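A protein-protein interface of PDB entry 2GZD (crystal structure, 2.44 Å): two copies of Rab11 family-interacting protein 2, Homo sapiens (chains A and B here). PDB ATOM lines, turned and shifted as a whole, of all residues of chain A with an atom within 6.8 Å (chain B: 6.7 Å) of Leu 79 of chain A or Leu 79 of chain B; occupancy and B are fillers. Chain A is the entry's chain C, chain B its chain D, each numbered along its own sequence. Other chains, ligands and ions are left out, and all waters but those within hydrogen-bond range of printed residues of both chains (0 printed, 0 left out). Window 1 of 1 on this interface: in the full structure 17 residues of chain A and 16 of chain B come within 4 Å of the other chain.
The backbone carbonyl oxygen of Ile 90 of chain A sits at hydrogen-bond distance from the guanidinium group of Arg 82 of chain B (2.5 Å).
CG2 of Ile 76 of chain B touches CE2 of Tyr 75 of chain A (3.6 Å). Ile 76 of chain A touches Tyr 75 of chain B (CG2 to CE2, 3.7 Å). Ile 76 of chain A touches Ile 76 of chain B (CG1 to CG1, 3.5 Å). Leu 79 of chain A touches Leu 79 of chain B (CD2 to CD2, 3.8 Å). Leu 79 of chain A touches Ile 90 of chain B. Leu 80 of chain A touches Tyr 75 of chain B (CD2 to OH, 3.6 Å). CD2 of Leu 80 of chain A touches CD2 of Leu 79 of chain B, at 3.6 Å. O of Ile 90 of chain B touches NE of Arg 82 of chain A, 3.6 Å away. Val 83 of chain A touches Val 83 of chain B (CG2 to CG2, 3.8 Å). CD1 of Leu 79 of chain B touches CD1 of Ile 90 of chain A, 3.3 Å away.
Asp 74 of chain A touches none of the printed residues of chain B. Printed residues of chain B within 4 Å of Leu 79 of chain A: Leu 79 and Ile 90. Leu 91 of chain A touches none of the printed residues of chain B. Of the printed residues of chain A, Ile 76 of chain B touches Tyr 75 and Ile 76. Leu 79 of chain B touches just these residues of chain A: Leu 79 (3.8 Å), Leu 80 (3.6 Å) and Ile 90 (3.3 Å). Printed residues of chain A within 4 Å of Leu 80 of chain B: Tyr 75 (3.7 Å). The nearest printed residue of chain B that does not touch Leu 79 of chain A is Leu 80 of chain B (4.02 Å). The nearest residue of chain A that does not touch Leu 79 of chain B is Leu 91 of chain A (4.1 Å).
Tyr 75 of chain A touches Ile 76 of chain B, and with the chains exchanged Ile 76 of chain A touches Tyr 75 of chain B. Tyr 75 of chain A touches Leu 80 of chain B, and with the chains exchanged Leu 80 of chain A touches Tyr 75 of chain B. Ile 76 of chain A touches its own counterpart, Ile 76 of chain B. Leu 80 of chain A touches Leu 79 of chain B, but with the chains exchanged Leu 79 of chain A does not touch Leu 80 of chain B (4.02 Å). 13 positions are printed for both chains. Of the 13 pairs that touch across the chains among the printed residues, 11 have their exchanged pair printed and touching as well.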
ATOM      1  N   ASP A  74      -9.810  26.930  37.504  1.00  0.00           N
ATOM      2  CA  ASP A  74     -10.978  27.792  37.725  1.00  0.00           C
ATOM      3  C   ASP A  74     -11.243  28.661  36.504  1.00  0.00           C
ATOM      4  O   ASP A  74     -12.376  29.025  36.215  1.00  0.00           O
ATOM      5  CB  ASP A  74     -10.749  28.727  38.925  1.00  0.00           C
ATOM      6  CG  ASP A  74     -10.804  28.014  40.259  1.00  0.00           C
ATOM      7  OD1 ASP A  74     -10.975  26.760  40.333  1.00  0.00           O
ATOM      8  OD2 ASP A  74     -10.678  28.748  41.244  1.00  0.00           O
ATOM      9  N   TYR A  75     -10.185  29.015  35.810  1.00  0.00           N
ATOM     10  CA  TYR A  75     -10.388  29.741  34.605  1.00  0.00           C
ATOM     11  C   TYR A  75     -11.102  28.852  33.570  1.00  0.00           C
ATOM     12  O   TYR A  75     -12.105  29.255  33.028  1.00  0.00           O
ATOM     13  CB  TYR A  75      -9.072  30.291  34.083  1.00  0.00           C
ATOM     14  CG  TYR A  75      -9.226  30.890  32.702  1.00  0.00           C
ATOM     15  CD1 TYR A  75      -9.520  32.252  32.535  1.00  0.00           C
ATOM     16  CD2 TYR A  75      -9.104  30.089  31.562  1.00  0.00           C
ATOM     17  CE1 TYR A  75      -9.668  32.804  31.298  1.00  0.00           C
ATOM     18  CE2 TYR A  75      -9.234  30.648  30.272  1.00  0.00           C
ATOM     19  CZ  TYR A  75      -9.506  32.025  30.156  1.00  0.00           C
ATOM     20  OH  TYR A  75      -9.648  32.593  28.891  1.00  0.00           O
ATOM     21  N   ILE A  76     -10.568  27.648  33.326  1.00  0.00           N
ATOM     22  CA  ILE A  76     -11.230  26.585  32.539  1.00  0.00           C
ATOM     23  C   ILE A  76     -12.719  26.427  32.967  1.00  0.00           C
ATOM     24  O   ILE A  76     -13.666  26.596  32.145  1.00  0.00           O
ATOM     25  CB  ILE A  76     -10.392  25.255  32.637  1.00  0.00           C
ATOM     26  CG1 ILE A  76      -9.000  25.469  31.999  1.00  0.00           C
ATOM     27  CG2 ILE A  76     -11.146  24.069  32.058  1.00  0.00           C
ATOM     28  CD1 ILE A  76      -7.941  24.345  32.298  1.00  0.00           C
ATOM     29  N   ASP A  77     -12.969  26.206  34.246  1.00  0.00           N
ATOM     30  CA  ASP A  77     -14.361  26.003  34.586  1.00  0.00           C
ATOM     31  C   ASP A  77     -15.230  27.199  34.197  1.00  0.00           C
ATOM     32  O   ASP A  77     -16.316  26.980  33.613  1.00  0.00           O
ATOM     33  CB  ASP A  77     -14.576  25.609  36.054  1.00  0.00           C
ATOM     34  CG  ASP A  77     -13.972  24.229  36.422  1.00  0.00           C
ATOM     35  OD1 ASP A  77     -13.884  23.305  35.539  1.00  0.00           O
ATOM     36  OD2 ASP A  77     -13.598  24.068  37.637  1.00  0.00           O
ATOM     37  N   ASN A  78     -14.808  28.455  34.505  1.00  0.00           N
ATOM     38  CA  ASN A  78     -15.717  29.603  34.226  1.00  0.00           C
ATOM     39  C   ASN A  78     -15.896  29.810  32.732  1.00  0.00           C
ATOM     40  O   ASN A  78     -16.951  30.194  32.279  1.00  0.00           O
ATOM     41  CB  ASN A  78     -15.340  30.933  34.920  1.00  0.00           C
ATOM     42  CG  ASN A  78     -15.240  30.815  36.444  1.00  0.00           C
ATOM     43  OD1 ASN A  78     -14.149  31.041  37.016  1.00  0.00           O
ATOM     44  ND2 ASN A  78     -16.362  30.465  37.115  1.00  0.00           N
ATOM     45  N   LEU A  79     -14.831  29.563  31.983  1.00  0.00           N
ATOM     46  CA  LEU A  79     -14.865  29.608  30.537  1.00  0.00           C
ATOM     47  C   LEU A  79     -15.837  28.517  29.994  1.00  0.00           C
ATOM     48  O   LEU A  79     -16.739  28.856  29.244  1.00  0.00           O
ATOM     49  CB  LEU A  79     -13.444  29.449  30.014  1.00  0.00           C
ATOM     50  CG  LEU A  79     -13.360  29.523  28.489  1.00  0.00           C
ATOM     51  CD1 LEU A  79     -14.133  30.748  27.890  1.00  0.00           C
ATOM     52  CD2 LEU A  79     -11.950  29.495  28.060  1.00  0.00           C
ATOM     53  N   LEU A  80     -15.694  27.247  30.447  1.00  0.00           N
ATOM     54  CA  LEU A  80     -16.542  26.128  29.998  1.00  0.00           C
ATOM     55  C   LEU A  80     -18.043  26.312  30.238  1.00  0.00           C
ATOM     56  O   LEU A  80     -18.878  25.931  29.377  1.00  0.00           O
ATOM     57  CB  LEU A  80     -16.040  24.789  30.546  1.00  0.00           C
ATOM     58  CG  LEU A  80     -14.684  24.325  29.954  1.00  0.00           C
ATOM     59  CD1 LEU A  80     -14.093  23.184  30.746  1.00  0.00           C
ATOM     60  CD2 LEU A  80     -14.747  23.965  28.465  1.00  0.00           C
ATOM     61  N   VAL A  81     -18.394  26.902  31.379  1.00  0.00           N
ATOM     62  CA  VAL A  81     -19.806  27.239  31.711  1.00  0.00           C
ATOM     63  C   VAL A  81     -20.440  28.045  30.560  1.00  0.00           C
ATOM     64  O   VAL A  81     -21.580  27.744  30.133  1.00  0.00           O
ATOM     65  CB  VAL A  81     -19.937  28.148  33.017  1.00  0.00           C
ATOM     66  CG1 VAL A  81     -21.360  28.639  33.199  1.00  0.00           C
ATOM     67  CG2 VAL A  81     -19.446  27.434  34.289  1.00  0.00           C
ATOM     68  N   ARG A  82     -19.702  29.067  30.104  1.00  0.00           N
ATOM     69  CA  ARG A  82     -20.126  29.972  29.047  1.00  0.00           C
ATOM     70  C   ARG A  82     -20.135  29.306  27.702  1.00  0.00           C
ATOM     71  O   ARG A  82     -21.078  29.495  26.926  1.00  0.00           O
ATOM     72  CB  ARG A  82     -19.203  31.188  28.996  1.00  0.00           C
ATOM     73  CG  ARG A  82     -19.401  32.095  30.204  1.00  0.00           C
ATOM     74  CD  ARG A  82     -18.699  33.402  30.025  1.00  0.00           C
ATOM     75  NE  ARG A  82     -17.250  33.213  29.962  1.00  0.00           N
ATOM     76  CZ  ARG A  82     -16.367  34.003  30.572  1.00  0.00           C
ATOM     77  NH1 ARG A  82     -16.821  35.038  31.292  1.00  0.00           N
ATOM     78  NH2 ARG A  82     -15.043  33.745  30.472  1.00  0.00           N
ATOM     79  N   VAL A  83     -19.072  28.535  27.422  1.00  0.00           N
ATOM     80  CA  VAL A  83     -19.019  27.663  26.258  1.00  0.00           C
ATOM     81  C   VAL A  83     -20.207  26.709  26.206  1.00  0.00           C
ATOM     82  O   VAL A  83     -20.874  26.642  25.181  1.00  0.00           O
ATOM     83  CB  VAL A  83     -17.657  26.936  26.111  1.00  0.00           C
ATOM     84  CG1 VAL A  83     -17.670  25.990  24.912  1.00  0.00           C
ATOM     85  CG2 VAL A  83     -16.547  27.936  25.925  1.00  0.00           C
ATOM     86  N   MET A  84     -20.510  26.030  27.309  1.00  0.00           N
ATOM     87  CA  MET A  84     -21.656  25.092  27.356  1.00  0.00           C
ATOM     88  C   MET A  84     -23.001  25.771  27.111  1.00  0.00           C
ATOM     89  O   MET A  84     -23.880  25.185  26.514  1.00  0.00           O
ATOM     90  CB  MET A  84     -21.708  24.288  28.680  1.00  0.00           C
ATOM     91  CG  MET A  84     -20.604  23.272  28.796  1.00  0.00           C
ATOM     92  SD  MET A  84     -20.112  22.730  30.676  1.00  0.00           S
ATOM     93  CE  MET A  84     -21.488  21.311  30.915  1.00  0.00           C
ATOM     94  N   ILE A  90     -18.489  23.239  20.357  1.00  0.00           N
ATOM     95  CA  ILE A  90     -17.031  23.310  20.360  1.00  0.00           C
ATOM     96  C   ILE A  90     -16.323  22.271  21.272  1.00  0.00           C
ATOM     97  O   ILE A  90     -15.114  22.059  21.138  1.00  0.00           O
ATOM     98  CB  ILE A  90     -16.420  24.777  20.651  1.00  0.00           C
ATOM     99  CG1 ILE A  90     -16.091  24.971  22.110  1.00  0.00           C
ATOM    100  CG2 ILE A  90     -17.167  25.961  20.023  1.00  0.00           C
ATOM    101  CD1 ILE A  90     -14.995  25.977  22.263  1.00  0.00           C
ATOM    102  N   LEU A  91     -17.076  21.657  22.189  1.00  0.00           N
ATOM    103  CA  LEU A  91     -16.571  20.596  23.091  1.00  0.00           C
ATOM    104  C   LEU A  91     -16.796  19.179  22.504  1.00  0.00           C
ATOM    105  O   LEU A  91     -16.551  18.169  23.182  1.00  0.00           O
ATOM    106  CB  LEU A  91     -17.226  20.688  24.503  1.00  0.00           C
ATOM    107  CG  LEU A  91     -17.366  22.086  25.178  1.00  0.00           C
ATOM    108  CD1 LEU A  91     -18.073  22.109  26.552  1.00  0.00           C
ATOM    109  CD2 LEU A  91     -15.988  22.737  25.285  1.00  0.00           C
ATOM    110  N   ASP B  74      -1.889  24.615  27.674  1.00  0.00           N
ATOM    111  CA  ASP B  74      -2.141  24.202  26.311  1.00  0.00           C
ATOM    112  C   ASP B  74      -3.601  23.913  26.096  1.00  0.00           C
ATOM    113  O   ASP B  74      -4.112  24.135  25.008  1.00  0.00           O
ATOM    114  CB  ASP B  74      -1.339  22.932  25.972  1.00  0.00           C
ATOM    115  CG  ASP B  74       0.173  23.173  25.887  1.00  0.00           C
ATOM    116  OD1 ASP B  74       0.668  24.181  26.427  1.00  0.00           O
ATOM    117  OD2 ASP B  74       0.866  22.352  25.252  1.00  0.00           O
ATOM    118  N   TYR B  75      -4.268  23.380  27.117  1.00  0.00           N
ATOM    119  CA  TYR B  75      -5.682  23.096  27.028  1.00  0.00           C
ATOM    120  C   TYR B  75      -6.404  24.445  26.814  1.00  0.00           C
ATOM    121  O   TYR B  75      -7.195  24.612  25.849  1.00  0.00           O
ATOM    122  CB  TYR B  75      -6.194  22.377  28.284  1.00  0.00           C
ATOM    123  CG  TYR B  75      -7.704  22.205  28.276  1.00  0.00           C
ATOM    124  CD1 TYR B  75      -8.308  21.105  27.648  1.00  0.00           C
ATOM    125  CD2 TYR B  75      -8.535  23.182  28.819  1.00  0.00           C
ATOM    126  CE1 TYR B  75      -9.698  20.970  27.596  1.00  0.00           C
ATOM    127  CE2 TYR B  75      -9.917  23.054  28.765  1.00  0.00           C
ATOM    128  CZ  TYR B  75     -10.486  21.945  28.170  1.00  0.00           C
ATOM    129  OH  TYR B  75     -11.855  21.862  28.122  1.00  0.00           O
ATOM    130  N   ILE B  76      -6.079  25.426  27.668  1.00  0.00           N
ATOM    131  CA  ILE B  76      -6.661  26.765  27.534  1.00  0.00           C
ATOM    132  C   ILE B  76      -6.507  27.320  26.128  1.00  0.00           C
ATOM    133  O   ILE B  76      -7.508  27.732  25.518  1.00  0.00           O
ATOM    134  CB  ILE B  76      -6.203  27.742  28.671  1.00  0.00           C
ATOM    135  CG1 ILE B  76      -6.878  27.380  30.017  1.00  0.00           C
ATOM    136  CG2 ILE B  76      -6.527  29.194  28.343  1.00  0.00           C
ATOM    137  CD1 ILE B  76      -5.899  27.386  31.205  1.00  0.00           C
ATOM    138  N   ASP B  77      -5.302  27.268  25.580  1.00  0.00           N
ATOM    139  CA  ASP B  77      -5.029  27.796  24.205  1.00  0.00           C
ATOM    140  C   ASP B  77      -5.742  27.152  23.039  1.00  0.00           C
ATOM    141  O   ASP B  77      -6.060  27.825  22.036  1.00  0.00           O
ATOM    142  CB  ASP B  77      -3.543  27.786  23.913  1.00  0.00           C
ATOM    143  CG  ASP B  77      -2.808  28.743  24.808  1.00  0.00           C
ATOM    144  OD1 ASP B  77      -3.503  29.624  25.410  1.00  0.00           O
ATOM    145  OD2 ASP B  77      -1.560  28.632  24.909  1.00  0.00           O
ATOM    146  N   ASN B  78      -5.954  25.840  23.163  1.00  0.00           N
ATOM    147  CA  ASN B  78      -6.677  25.063  22.179  1.00  0.00           C
ATOM    148  C   ASN B  78      -8.152  25.391  22.274  1.00  0.00           C
ATOM    149  O   ASN B  78      -8.816  25.640  21.291  1.00  0.00           O
ATOM    150  CB  ASN B  78      -6.387  23.585  22.417  1.00  0.00           C
ATOM    151  CG  ASN B  78      -4.969  23.173  21.934  1.00  0.00           C
ATOM    152  OD1 ASN B  78      -4.353  22.276  22.507  1.00  0.00           O
ATOM    153  ND2 ASN B  78      -4.463  23.825  20.881  1.00  0.00           N
ATOM    154  N   LEU B  79      -8.642  25.457  23.497  1.00  0.00           N
ATOM    155  CA  LEU B  79     -10.005  25.842  23.718  1.00  0.00           C
ATOM    156  C   LEU B  79     -10.242  27.270  23.153  1.00  0.00           C
ATOM    157  O   LEU B  79     -11.161  27.489  22.351  1.00  0.00           O
ATOM    158  CB  LEU B  79     -10.359  25.683  25.207  1.00  0.00           C
ATOM    159  CG  LEU B  79     -11.812  26.055  25.533  1.00  0.00           C
ATOM    160  CD1 LEU B  79     -12.792  25.298  24.668  1.00  0.00           C
ATOM    161  CD2 LEU B  79     -12.146  25.857  26.960  1.00  0.00           C
ATOM    162  N   LEU B  80      -9.384  28.217  23.538  1.00  0.00           N
ATOM    163  CA  LEU B  80      -9.516  29.606  23.117  1.00  0.00           C
ATOM    164  C   LEU B  80      -9.461  29.814  21.618  1.00  0.00           C
ATOM    165  O   LEU B  80     -10.165  30.667  21.122  1.00  0.00           O
ATOM    166  CB  LEU B  80      -8.447  30.457  23.799  1.00  0.00           C
ATOM    167  CG  LEU B  80      -8.738  30.790  25.257  1.00  0.00           C
ATOM    168  CD1 LEU B  80      -7.542  31.370  25.997  1.00  0.00           C
ATOM    169  CD2 LEU B  80      -9.958  31.675  25.336  1.00  0.00           C
ATOM    170  N   VAL B  81      -8.599  29.077  20.901  1.00  0.00           N
ATOM    171  CA  VAL B  81      -8.543  29.103  19.422  1.00  0.00           C
ATOM    172  C   VAL B  81      -9.932  28.839  18.828  1.00  0.00           C
ATOM    173  O   VAL B  81     -10.359  29.547  17.929  1.00  0.00           O
ATOM    174  CB  VAL B  81      -7.549  28.031  18.833  1.00  0.00           C
ATOM    175  CG1 VAL B  81      -7.571  28.029  17.280  1.00  0.00           C
ATOM    176  CG2 VAL B  81      -6.184  28.281  19.285  1.00  0.00           C
ATOM    177  N   ARG B  82     -10.617  27.809  19.341  1.00  0.00           N
ATOM    178  CA  ARG B  82     -12.007  27.477  18.953  1.00  0.00           C
ATOM    179  C   ARG B  82     -13.025  28.549  19.330  1.00  0.00           C
ATOM    180  O   ARG B  82     -13.920  28.843  18.537  1.00  0.00           O
ATOM    181  CB  ARG B  82     -12.449  26.110  19.500  1.00  0.00           C
ATOM    182  CG  ARG B  82     -11.661  24.918  18.939  1.00  0.00           C
ATOM    183  CD  ARG B  82     -12.124  23.601  19.589  1.00  0.00           C
ATOM    184  NE  ARG B  82     -11.747  23.396  21.017  1.00  0.00           N
ATOM    185  CZ  ARG B  82     -12.058  22.296  21.741  1.00  0.00           C
ATOM    186  NH1 ARG B  82     -12.762  21.311  21.158  1.00  0.00           N
ATOM    187  NH2 ARG B  82     -11.690  22.153  23.033  1.00  0.00           N
ATOM    188  N   VAL B  83     -12.910  29.088  20.556  1.00  0.00           N
ATOM    189  CA  VAL B  83     -13.806  30.144  21.044  1.00  0.00           C
ATOM    190  C   VAL B  83     -13.639  31.432  20.210  1.00  0.00           C
ATOM    191  O   VAL B  83     -14.626  32.000  19.737  1.00  0.00           O
ATOM    192  CB  VAL B  83     -13.613  30.472  22.521  1.00  0.00           C
ATOM    193  CG1 VAL B  83     -14.362  31.741  22.865  1.00  0.00           C
ATOM    194  CG2 VAL B  83     -14.083  29.349  23.414  1.00  0.00           C
ATOM    195  N   MET B  84     -12.404  31.858  20.013  1.00  0.00           N
ATOM    196  CA  MET B  84     -12.089  33.021  19.204  1.00  0.00           C
ATOM    197  C   MET B  84     -12.628  32.909  17.802  1.00  0.00           C
ATOM    198  O   MET B  84     -13.004  33.895  17.231  1.00  0.00           O
ATOM    199  CB  MET B  84     -10.571  33.229  19.123  1.00  0.00           C
ATOM    200  CG  MET B  84      -9.994  33.602  20.453  1.00  0.00           C
ATOM    201  SD  MET B  84      -8.034  33.516  20.581  1.00  0.00           S
ATOM    202  CE  MET B  84      -7.609  35.346  19.655  1.00  0.00           C
ATOM    203  N   ILE B  90     -17.727  35.650  23.768  1.00  0.00           N
ATOM    204  CA  ILE B  90     -17.668  35.029  25.128  1.00  0.00           C
ATOM    205  C   ILE B  90     -16.422  35.453  25.963  1.00  0.00           C
ATOM    206  O   ILE B  90     -16.376  35.294  27.169  1.00  0.00           O
ATOM    207  CB  ILE B  90     -18.027  33.475  25.155  1.00  0.00           C
ATOM    208  CG1 ILE B  90     -17.202  32.707  26.187  1.00  0.00           C
ATOM    209  CG2 ILE B  90     -17.909  32.814  23.788  1.00  0.00           C
ATOM    210  CD1 ILE B  90     -15.831  32.330  25.753  1.00  0.00           C
ATOM    211  N   LEU B  91     -15.459  36.049  25.268  1.00  0.00           N
ATOM    212  CA  LEU B  91     -14.213  36.541  25.832  1.00  0.00           C
ATOM    213  C   LEU B  91     -14.258  38.057  26.022  1.00  0.00           C
ATOM    214  O   LEU B  91     -13.247  38.651  26.341  1.00  0.00           O
ATOM    215  CB  LEU B  91     -13.067  36.187  24.892  1.00  0.00           C
ATOM    216  CG  LEU B  91     -12.921  34.733  24.453  1.00  0.00           C
ATOM    217  CD1 LEU B  91     -11.816  34.595  23.394  1.00  0.00           C
ATOM    218  CD2 LEU B  91     -12.647  33.886  25.675  1.00  0.00           C
